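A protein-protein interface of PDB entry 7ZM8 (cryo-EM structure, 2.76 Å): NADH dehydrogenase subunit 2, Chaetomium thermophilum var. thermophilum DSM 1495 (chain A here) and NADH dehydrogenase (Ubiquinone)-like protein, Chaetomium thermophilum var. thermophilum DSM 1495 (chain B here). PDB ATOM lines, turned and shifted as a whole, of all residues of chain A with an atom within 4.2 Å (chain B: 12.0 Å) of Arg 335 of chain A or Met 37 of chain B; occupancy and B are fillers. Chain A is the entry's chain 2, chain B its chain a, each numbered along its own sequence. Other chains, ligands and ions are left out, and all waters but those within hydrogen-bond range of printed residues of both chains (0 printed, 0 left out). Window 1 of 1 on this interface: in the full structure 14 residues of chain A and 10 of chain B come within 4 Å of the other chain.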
ATOM      1  N   LEU A 171      21.925  40.744 -12.683  1.00  0.00           N
ATOM      2  CA  LEU A 171      21.444  40.425 -11.323  1.00  0.00           C
ATOM      3  C   LEU A 171      21.455  41.710 -10.516  1.00  0.00           C
ATOM      4  O   LEU A 171      20.538  41.901  -9.715  1.00  0.00           O
ATOM      5  CB  LEU A 171      22.335  39.355 -10.691  1.00  0.00           C
ATOM      6  CG  LEU A 171      22.015  37.918 -11.087  1.00  0.00           C
ATOM      7  CD1 LEU A 171      22.856  36.952 -10.278  1.00  0.00           C
ATOM      8  CD2 LEU A 171      20.539  37.631 -10.899  1.00  0.00           C
ATOM      9  N   ASP A 269      21.089  38.795  -2.276  1.00  0.00           N
ATOM     10  CA  ASP A 269      21.594  37.693  -3.085  1.00  0.00           C
ATOM     11  C   ASP A 269      22.000  38.141  -4.482  1.00  0.00           C
ATOM     12  O   ASP A 269      22.897  37.544  -5.082  1.00  0.00           O
ATOM     13  CB  ASP A 269      20.525  36.604  -3.174  1.00  0.00           C
ATOM     14  CG  ASP A 269      21.093  35.245  -3.512  1.00  0.00           C
ATOM     15  OD1 ASP A 269      22.103  34.846  -2.902  1.00  0.00           O
ATOM     16  OD2 ASP A 269      20.512  34.568  -4.388  1.00  0.00           O
ATOM     17  N   GLN A 333      17.396  27.190   3.285  1.00  0.00           N
ATOM     18  CA  GLN A 333      18.162  28.003   2.360  1.00  0.00           C
ATOM     19  C   GLN A 333      19.439  27.266   1.987  1.00  0.00           C
ATOM     20  O   GLN A 333      20.106  26.694   2.852  1.00  0.00           O
ATOM     21  CB  GLN A 333      18.481  29.369   2.970  1.00  0.00           C
ATOM     22  CG  GLN A 333      17.251  30.149   3.396  1.00  0.00           C
ATOM     23  CD  GLN A 333      16.326  30.455   2.237  1.00  0.00           C
ATOM     24  OE1 GLN A 333      16.631  31.292   1.395  1.00  0.00           O
ATOM     25  NE2 GLN A 333      15.189  29.776   2.188  1.00  0.00           N
ATOM     26  N   PHE A 334      19.754  27.253   0.697  1.00  0.00           N
ATOM     27  CA  PHE A 334      20.992  26.672   0.213  1.00  0.00           C
ATOM     28  C   PHE A 334      21.936  27.704  -0.380  1.00  0.00           C
ATOM     29  O   PHE A 334      23.076  27.362  -0.703  1.00  0.00           O
ATOM     30  CB  PHE A 334      20.702  25.581  -0.827  1.00  0.00           C
ATOM     31  CG  PHE A 334      20.122  26.105  -2.096  1.00  0.00           C
ATOM     32  CD1 PHE A 334      18.769  26.332  -2.203  1.00  0.00           C
ATOM     33  CD2 PHE A 334      20.930  26.382  -3.179  1.00  0.00           C
ATOM     34  CE1 PHE A 334      18.239  26.821  -3.348  1.00  0.00           C
ATOM     35  CE2 PHE A 334      20.396  26.876  -4.330  1.00  0.00           C
ATOM     36  CZ  PHE A 334      19.047  27.097  -4.411  1.00  0.00           C
ATOM     37  N   ARG A 335      21.498  28.945  -0.530  1.00  0.00           N
ATOM     38  CA  ARG A 335      22.339  30.025  -1.017  1.00  0.00           C
ATOM     39  C   ARG A 335      22.817  30.855   0.168  1.00  0.00           C
ATOM     40  O   ARG A 335      22.016  31.248   1.018  1.00  0.00           O
ATOM     41  CB  ARG A 335      21.578  30.882  -2.029  1.00  0.00           C
ATOM     42  CG  ARG A 335      21.302  30.146  -3.325  1.00  0.00           C
ATOM     43  CD  ARG A 335      20.723  31.032  -4.397  1.00  0.00           C
ATOM     44  NE  ARG A 335      21.652  32.071  -4.812  1.00  0.00           N
ATOM     45  CZ  ARG A 335      22.510  31.957  -5.813  1.00  0.00           C
ATOM     46  NH1 ARG A 335      23.310  32.965  -6.107  1.00  0.00           N
ATOM     47  NH2 ARG A 335      22.566  30.845  -6.523  1.00  0.00           N
ATOM     48  N   ILE A 336      24.122  31.113   0.219  1.00  0.00           N
ATOM     49  CA  ILE A 336      24.738  31.649   1.427  1.00  0.00           C
ATOM     50  C   ILE A 336      24.290  33.085   1.692  1.00  0.00           C
ATOM     51  O   ILE A 336      24.116  33.484   2.847  1.00  0.00           O
ATOM     52  CB  ILE A 336      26.274  31.511   1.347  1.00  0.00           C
ATOM     53  CG1 ILE A 336      26.924  31.872   2.685  1.00  0.00           C
ATOM     54  CG2 ILE A 336      26.860  32.333   0.220  1.00  0.00           C
ATOM     55  CD1 ILE A 336      26.529  30.976   3.825  1.00  0.00           C
ATOM     56  N   LYS A 337      24.104  33.889   0.645  1.00  0.00           N
ATOM     57  CA  LYS A 337      23.688  35.269   0.863  1.00  0.00           C
ATOM     58  C   LYS A 337      22.214  35.374   1.221  1.00  0.00           C
ATOM     59  O   LYS A 337      21.822  36.307   1.925  1.00  0.00           O
ATOM     60  CB  LYS A 337      24.002  36.127  -0.364  1.00  0.00           C
ATOM     61  CG  LYS A 337      25.483  36.245  -0.667  1.00  0.00           C
ATOM     62  CD  LYS A 337      25.742  36.683  -2.095  1.00  0.00           C
ATOM     63  CE  LYS A 337      25.913  38.184  -2.187  1.00  0.00           C
ATOM     64  NZ  LYS A 337      25.574  38.727  -3.527  1.00  0.00           N
ATOM     65  N   ARG A 338      21.382  34.450   0.738  1.00  0.00           N
ATOM     66  CA  ARG A 338      20.012  34.369   1.230  1.00  0.00           C
ATOM     67  C   ARG A 338      19.982  33.950   2.692  1.00  0.00           C
ATOM     68  O   ARG A 338      19.146  34.424   3.466  1.00  0.00           O
ATOM     69  CB  ARG A 338      19.196  33.396   0.385  1.00  0.00           C
ATOM     70  CG  ARG A 338      19.120  33.759  -1.071  1.00  0.00           C
ATOM     71  CD  ARG A 338      18.031  32.990  -1.774  1.00  0.00           C
ATOM     72  NE  ARG A 338      16.729  33.188  -1.151  1.00  0.00           N
ATOM     73  CZ  ARG A 338      15.877  34.145  -1.494  1.00  0.00           C
ATOM     74  NH1 ARG A 338      16.188  35.000  -2.457  1.00  0.00           N
ATOM     75  NH2 ARG A 338      14.715  34.250  -0.869  1.00  0.00           N
ATOM     76  N   LEU A 339      20.884  33.048   3.084  1.00  0.00           N
ATOM     77  CA  LEU A 339      20.955  32.625   4.475  1.00  0.00           C
ATOM     78  C   LEU A 339      21.379  33.765   5.385  1.00  0.00           C
ATOM     79  O   LEU A 339      20.808  33.948   6.465  1.00  0.00           O
ATOM     80  CB  LEU A 339      21.922  31.457   4.616  1.00  0.00           C
ATOM     81  CG  LEU A 339      21.916  30.833   6.007  1.00  0.00           C
ATOM     82  CD1 LEU A 339      20.680  29.993   6.164  1.00  0.00           C
ATOM     83  CD2 LEU A 339      23.146  30.010   6.242  1.00  0.00           C
ATOM     84  N   GLN A 413      28.411  31.599  -3.901  1.00  0.00           N
ATOM     85  CA  GLN A 413      26.967  31.740  -3.864  1.00  0.00           C
ATOM     86  C   GLN A 413      26.263  30.594  -3.170  1.00  0.00           C
ATOM     87  O   GLN A 413      25.168  30.792  -2.647  1.00  0.00           O
ATOM     88  CB  GLN A 413      26.397  31.872  -5.283  1.00  0.00           C
ATOM     89  CG  GLN A 413      26.798  33.129  -5.996  1.00  0.00           C
ATOM     90  CD  GLN A 413      26.669  33.011  -7.494  1.00  0.00           C
ATOM     91  OE1 GLN A 413      25.616  32.657  -8.009  1.00  0.00           O
ATOM     92  NE2 GLN A 413      27.742  33.326  -8.207  1.00  0.00           N
ATOM     93  N   LEU A 414      26.858  29.408  -3.150  1.00  0.00           N
ATOM     94  CA  LEU A 414      26.265  28.238  -2.532  1.00  0.00           C
ATOM     95  C   LEU A 414      27.044  27.853  -1.287  1.00  0.00           C
ATOM     96  O   LEU A 414      28.259  28.042  -1.209  1.00  0.00           O
ATOM     97  CB  LEU A 414      26.231  27.061  -3.508  1.00  0.00           C
ATOM     98  CG  LEU A 414      25.594  27.342  -4.870  1.00  0.00           C
ATOM     99  CD1 LEU A 414      25.712  26.134  -5.770  1.00  0.00           C
ATOM    100  CD2 LEU A 414      24.142  27.759  -4.715  1.00  0.00           C
ATOM    101  N   PHE B  32      11.406  38.597 -11.201  1.00  0.00           N
ATOM    102  CA  PHE B  32      12.518  39.293 -11.899  1.00  0.00           C
ATOM    103  C   PHE B  32      13.784  38.437 -11.843  1.00  0.00           C
ATOM    104  O   PHE B  32      14.622  38.550 -12.750  1.00  0.00           O
ATOM    105  CB  PHE B  32      12.691  40.729 -11.399  1.00  0.00           C
ATOM    106  CG  PHE B  32      11.870  41.748 -12.147  1.00  0.00           C
ATOM    107  CD1 PHE B  32      11.437  41.495 -13.439  1.00  0.00           C
ATOM    108  CD2 PHE B  32      11.533  42.959 -11.564  1.00  0.00           C
ATOM    109  CE1 PHE B  32      10.683  42.428 -14.131  1.00  0.00           C
ATOM    110  CE2 PHE B  32      10.776  43.890 -12.257  1.00  0.00           C
ATOM    111  CZ  PHE B  32      10.358  43.626 -13.539  1.00  0.00           C
ATOM    112  N   LEU B  33      13.920  37.614 -10.802  1.00  0.00           N
ATOM    113  CA  LEU B  33      15.176  36.845 -10.630  1.00  0.00           C
ATOM    114  C   LEU B  33      15.080  35.445 -11.262  1.00  0.00           C
ATOM    115  O   LEU B  33      13.951  35.019 -11.528  1.00  0.00           O
ATOM    116  CB  LEU B  33      15.561  36.797  -9.152  1.00  0.00           C
ATOM    117  CG  LEU B  33      16.050  38.116  -8.562  1.00  0.00           C
ATOM    118  CD1 LEU B  33      16.115  38.041  -7.047  1.00  0.00           C
ATOM    119  CD2 LEU B  33      17.405  38.490  -9.135  1.00  0.00           C
ATOM    120  N   PRO B  34      16.199  34.720 -11.542  1.00  0.00           N
ATOM    121  CA  PRO B  34      16.118  33.365 -12.089  1.00  0.00           C
ATOM    122  C   PRO B  34      15.467  32.400 -11.116  1.00  0.00           C
ATOM    123  O   PRO B  34      15.502  32.588  -9.898  1.00  0.00           O
ATOM    124  CB  PRO B  34      17.583  32.991 -12.332  1.00  0.00           C
ATOM    125  CG  PRO B  34      18.310  34.277 -12.353  1.00  0.00           C
ATOM    126  CD  PRO B  34      17.592  35.177 -11.425  1.00  0.00           C
ATOM    127  N   GLU B  35      14.857  31.355 -11.676  1.00  0.00           N
ATOM    128  CA  GLU B  35      14.260  30.310 -10.856  1.00  0.00           C
ATOM    129  C   GLU B  35      15.305  29.487 -10.120  1.00  0.00           C
ATOM    130  O   GLU B  35      14.989  28.875  -9.099  1.00  0.00           O
ATOM    131  CB  GLU B  35      13.393  29.395 -11.722  1.00  0.00           C
ATOM    132  CG  GLU B  35      12.107  30.042 -12.206  1.00  0.00           C
ATOM    133  CD  GLU B  35      11.114  30.269 -11.083  1.00  0.00           C
ATOM    134  OE1 GLU B  35      11.069  29.437 -10.153  1.00  0.00           O
ATOM    135  OE2 GLU B  35      10.382  31.279 -11.128  1.00  0.00           O
ATOM    136  N   ALA B  36      16.539  29.463 -10.618  1.00  0.00           N
ATOM    137  CA  ALA B  36      17.619  28.768  -9.937  1.00  0.00           C
ATOM    138  C   ALA B  36      17.990  29.424  -8.617  1.00  0.00           C
ATOM    139  O   ALA B  36      18.605  28.774  -7.768  1.00  0.00           O
ATOM    140  CB  ALA B  36      18.846  28.711 -10.844  1.00  0.00           C
ATOM    141  N   MET B  37      17.637  30.692  -8.430  1.00  0.00           N
ATOM    142  CA  MET B  37      18.065  31.463  -7.274  1.00  0.00           C
ATOM    143  C   MET B  37      16.982  31.669  -6.231  1.00  0.00           C
ATOM    144  O   MET B  37      17.304  31.761  -5.045  1.00  0.00           O
ATOM    145  CB  MET B  37      18.578  32.836  -7.722  1.00  0.00           C
ATOM    146  CG  MET B  37      19.850  32.785  -8.539  1.00  0.00           C
ATOM    147  SD  MET B  37      20.361  34.405  -9.109  1.00  0.00           S
ATOM    148  CE  MET B  37      20.893  35.182  -7.591  1.00  0.00           C
ATOM    149  N   VAL B  38      15.717  31.753  -6.629  1.00  0.00           N
ATOM    150  CA  VAL B  38      14.643  32.045  -5.686  1.00  0.00           C
ATOM    151  C   VAL B  38      13.529  31.018  -5.834  1.00  0.00           C
ATOM    152  O   VAL B  38      12.622  30.951  -4.999  1.00  0.00           O
ATOM    153  CB  VAL B  38      14.093  33.473  -5.881  1.00  0.00           C
ATOM    154  CG1 VAL B  38      15.211  34.487  -5.861  1.00  0.00           C
ATOM    155  CG2 VAL B  38      13.315  33.575  -7.184  1.00  0.00           C
ATOM    156  N   GLY B  39      13.590  30.212  -6.889  1.00  0.00           N
ATOM    157  CA  GLY B  39      12.519  29.272  -7.153  1.00  0.00           C
ATOM    158  C   GLY B  39      12.402  28.200  -6.085  1.00  0.00           C
ATOM    159  O   GLY B  39      13.389  27.752  -5.503  1.00  0.00           O
ATOM    160  N   ARG B  40      11.159  27.790  -5.821  1.00  0.00           N
ATOM    161  CA  ARG B  40      10.916  26.670  -4.920  1.00  0.00           C
ATOM    162  C   ARG B  40      11.425  25.359  -5.500  1.00  0.00           C
ATOM    163  O   ARG B  40      11.697  24.422  -4.743  1.00  0.00           O
ATOM    164  CB  ARG B  40       9.418  26.550  -4.611  1.00  0.00           C
ATOM    165  CG  ARG B  40       9.075  25.450  -3.612  1.00  0.00           C
ATOM    166  CD  ARG B  40       7.594  25.108  -3.589  1.00  0.00           C
ATOM    167  NE  ARG B  40       7.329  23.949  -2.737  1.00  0.00           N
ATOM    168  CZ  ARG B  40       7.016  24.021  -1.447  1.00  0.00           C
ATOM    169  NH1 ARG B  40       6.905  25.199  -0.860  1.00  0.00           N
ATOM    170  NH2 ARG B  40       6.798  22.918  -0.747  1.00  0.00           N
ATOM    171  N   SER B  41      11.580  25.286  -6.822  1.00  0.00           N
ATOM    172  CA  SER B  41      11.919  24.026  -7.471  1.00  0.00           C
ATOM    173  C   SER B  41      13.261  23.491  -6.995  1.00  0.00           C
ATOM    174  O   SER B  41      13.420  22.281  -6.805  1.00  0.00           O
ATOM    175  CB  SER B  41      11.924  24.208  -8.988  1.00  0.00           C
ATOM    176  OG  SER B  41      12.358  23.029  -9.641  1.00  0.00           O
ATOM    177  N   LYS B  42      14.243  24.367  -6.805  1.00  0.00           N
ATOM    178  CA  LYS B  42      15.560  23.890  -6.413  1.00  0.00           C
ATOM    179  C   LYS B  42      15.686  23.736  -4.905  1.00  0.00           C
ATOM    180  O   LYS B  42      16.634  23.102  -4.433  1.00  0.00           O
ATOM    181  CB  LYS B  42      16.638  24.820  -6.989  1.00  0.00           C
ATOM    182  CG  LYS B  42      18.060  24.352  -6.768  1.00  0.00           C
ATOM    183  CD  LYS B  42      19.064  25.335  -7.306  1.00  0.00           C
ATOM    184  CE  LYS B  42      19.106  25.291  -8.823  1.00  0.00           C
ATOM    185  NZ  LYS B  42      20.175  26.168  -9.372  1.00  0.00           N
ATOM    186  N   ILE B  43      14.740  24.279  -4.140  1.00  0.00           N
ATOM    187  CA  ILE B  43      14.597  23.864  -2.748  1.00  0.00           C
ATOM    188  C   ILE B  43      14.188  22.400  -2.686  1.00  0.00           C
ATOM    189  O   ILE B  43      14.723  21.620  -1.890  1.00  0.00           O
ATOM    190  CB  ILE B  43      13.584  24.762  -2.019  1.00  0.00           C
ATOM    191  CG1 ILE B  43      14.029  26.224  -2.064  1.00  0.00           C
ATOM    192  CG2 ILE B  43      13.438  24.320  -0.584  1.00  0.00           C
ATOM    193  CD1 ILE B  43      15.344  26.483  -1.398  1.00  0.00           C
ATOM    194  N   ASP B  44      13.256  21.998  -3.549  1.00  0.00           N
ATOM    195  CA  ASP B  44      12.765  20.630  -3.593  1.00  0.00           C
ATOM    196  C   ASP B  44      13.825  19.623  -4.015  1.00  0.00           C
ATOM    197  O   ASP B  44      13.608  18.421  -3.849  1.00  0.00           O
ATOM    198  CB  ASP B  44      11.568  20.548  -4.537  1.00  0.00           C
ATOM    199  CG  ASP B  44      10.278  20.989  -3.877  1.00  0.00           C
ATOM    200  OD1 ASP B  44      10.347  21.707  -2.858  1.00  0.00           O
ATOM    201  OD2 ASP B  44       9.193  20.618  -4.378  1.00  0.00           O
ATOM    202  N   GLU B  45      14.948  20.072  -4.569  1.00  0.00           N
ATOM    203  CA  GLU B  45      16.067  19.181  -4.838  1.00  0.00           C
ATOM    204  C   GLU B  45      17.027  19.113  -3.660  1.00  0.00           C
ATOM    205  O   GLU B  45      17.596  18.054  -3.381  1.00  0.00           O
ATOM    206  CB  GLU B  45      16.815  19.635  -6.093  1.00  0.00           C
ATOM    207  CG  GLU B  45      17.664  18.549  -6.740  1.00  0.00           C
ATOM    208  CD  GLU B  45      18.000  18.856  -8.186  1.00  0.00           C
ATOM    209  OE1 GLU B  45      17.144  19.430  -8.890  1.00  0.00           O
ATOM    210  OE2 GLU B  45      19.124  18.525  -8.618  1.00  0.00           O
ATOM    211  N   LYS B  46      17.217  20.232  -2.963  1.00  0.00           N
ATOM    212  CA  LYS B  46      18.077  20.238  -1.787  1.00  0.00           C
ATOM    213  C   LYS B  46      17.386  19.568  -0.608  1.00  0.00           C
ATOM    214  O   LYS B  46      18.031  18.893   0.201  1.00  0.00           O
ATOM    215  CB  LYS B  46      18.445  21.673  -1.422  1.00  0.00           C
ATOM    216  CG  LYS B  46      19.177  22.437  -2.490  1.00  0.00           C
ATOM    217  CD  LYS B  46      20.544  21.876  -2.786  1.00  0.00           C
ATOM    218  CE  LYS B  46      21.274  22.799  -3.741  1.00  0.00           C
ATOM    219  NZ  LYS B  46      20.645  22.777  -5.088  1.00  0.00           N
ATOM    220  N   TYR B  47      16.077  19.760  -0.490  1.00  0.00           N
ATOM    221  CA  TYR B  47      15.289  19.273   0.637  1.00  0.00           C
ATOM    222  C   TYR B  47      14.052  18.562   0.107  1.00  0.00           C
ATOM    223  O   TYR B  47      12.922  19.012   0.326  1.00  0.00           O
ATOM    224  CB  TYR B  47      14.908  20.427   1.565  1.00  0.00           C
ATOM    225  CG  TYR B  47      16.098  21.183   2.108  1.00  0.00           C
ATOM    226  CD1 TYR B  47      16.751  20.750   3.250  1.00  0.00           C
ATOM    227  CD2 TYR B  47      16.573  22.322   1.475  1.00  0.00           C
ATOM    228  CE1 TYR B  47      17.836  21.426   3.746  1.00  0.00           C
ATOM    229  CE2 TYR B  47      17.660  23.006   1.965  1.00  0.00           C
ATOM    230  CZ  TYR B  47      18.288  22.554   3.102  1.00  0.00           C
ATOM    231  OH  TYR B  47      19.376  23.229   3.607  1.00  0.00           O
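Leu 171 of chain A touches just these residues of chain B: Leu 33, Pro 34 and Met 37.
Asp 269 of chain A touches just one residue of chain B: Met 37.
Of chain B, only Tyr 47 (3.6 Å) comes within 4 Å of Gln 333 of chain A.
Of chain B, only Ala 36 (3.8 Å), Lys 42 (3.4 Å), Ile 43 (3.5 Å) and Lys 46 (3.6 Å) come within 4 Å of Phe 334 of chain A.
Arg 335 of chain A touches one residue of chain B.
No residue of chain B comes within 4 Å of Lys 337 of chain A.
Arg 338 of chain A touches just these residues of chain B: Met 37 (3.6 Å) and Val 38 (3.6 Å).
No residue of chain B comes within 4 Å of Gln 413 of chain A.
Met 37 of chain B touches four residues of chain A.
Printed residues of chain A within 4 Å of Lys 42 of chain B: Phe 334 (3.4 Å).
Of the printed residues of chain A, Ile 43 of chain B touches Phe 334.
Of the printed residues of chain A, Lys 46 of chain B touches Phe 334 (3.6 Å).
The nearest residue of chain B that does not touch Arg 335 of chain A is Ala 36 of chain B (4.6 Å).
The nearest printed residue of chain A that does not touch Met 37 of chain B is Phe 334 of chain A (5.0 Å).
The nearest printed residue of chain A that does not touch Leu 33 of chain B is Arg 338 of chain A (5.5 Å).
The guanidinium group (NH1) of Arg 335 of chain A sits at hydrogen-bond distance from the side-chain amide oxygen (OE1) of Gln 413 of chain A, 3.0 Å away.
The backbone carbonyl oxygen of Asp 269 of chain A sits at hydrogen-bond distance from the side-chain amino group of Lys 337 of chain A (3.3 Å).
The side-chain amide oxygen of Gln 333 of chain A lies within hydrogen-bond range of the guanidinium group of Arg 338 of chain A.
The guanidinium group (NE) of Arg 335 of chain A lies within salt-bridge range of the side-chain carboxylate (OD2) of Asp 269 of chain A, at 2.8 Å.
The backbone carbonyl oxygen (O) of Ala 36 of chain B sits close to the side-chain amino group (NZ) of Lys 42 of chain B (3.4 Å).
Leu 171 of chain A touches Leu 33 of chain B (CD2 to CD2, 3.7 Å).
Pro 34 of chain B touches Leu 171 of chain A (CD to CD2, 3.9 Å).
Leu 171 of chain A touches Met 37 of chain B (CD2 to SD, 3.7 Å).
Met 37 of chain B touches Asp 269 of chain A.
CZ of Phe 334 of chain A touches CD of Lys 42 of chain B, at 3.4 Å.
Phe 334 of chain A touches Ile 43 of chain B (CE1 to CD1, 3.5 Å).
CE of Lys 46 of chain B touches CD2 of Phe 334 of chain A (3.6 Å).
Met 37 of chain B touches Arg 335 of chain A (O to CD, 3.6 Å).
CD of Arg 338 of chain A touches O of Met 37 of chain B (3.6 Å).
Arg 338 of chain A touches Val 38 of chain B.
Printed residues of chain B that touch a printed residue of chain A: Leu 33, Pro 34, Ala 36, Met 37, Val 38, Lys 42, Ile 43, Lys 46 and Tyr 47.
Hydrophobic or aromatic side chains of chain B within 4 Å of the printed part of chain A: Leu 33, Pro 34, Met 37, Val 38, Ile 43 and Tyr 47.
Along chain B the printed residues that touch a printed residue of chain A span positions 33 to 47.
Of the 11 printed residues of chain A, 6 touch a printed residue of chain B.
Printed residues of chain A that touch a printed residue of chain B: Leu 171, Asp 269, Gln 333, Phe 334, Arg 335 and Arg 338.
Hydrophobic or aromatic side chains of chain A within 4 Å of the printed part of chain B: Leu 171 and Phe 334.
Among the printed residues, no Asp or Glu carboxylate lies within 4 Å of a Lys or Arg side-chain nitrogen of the other chain.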
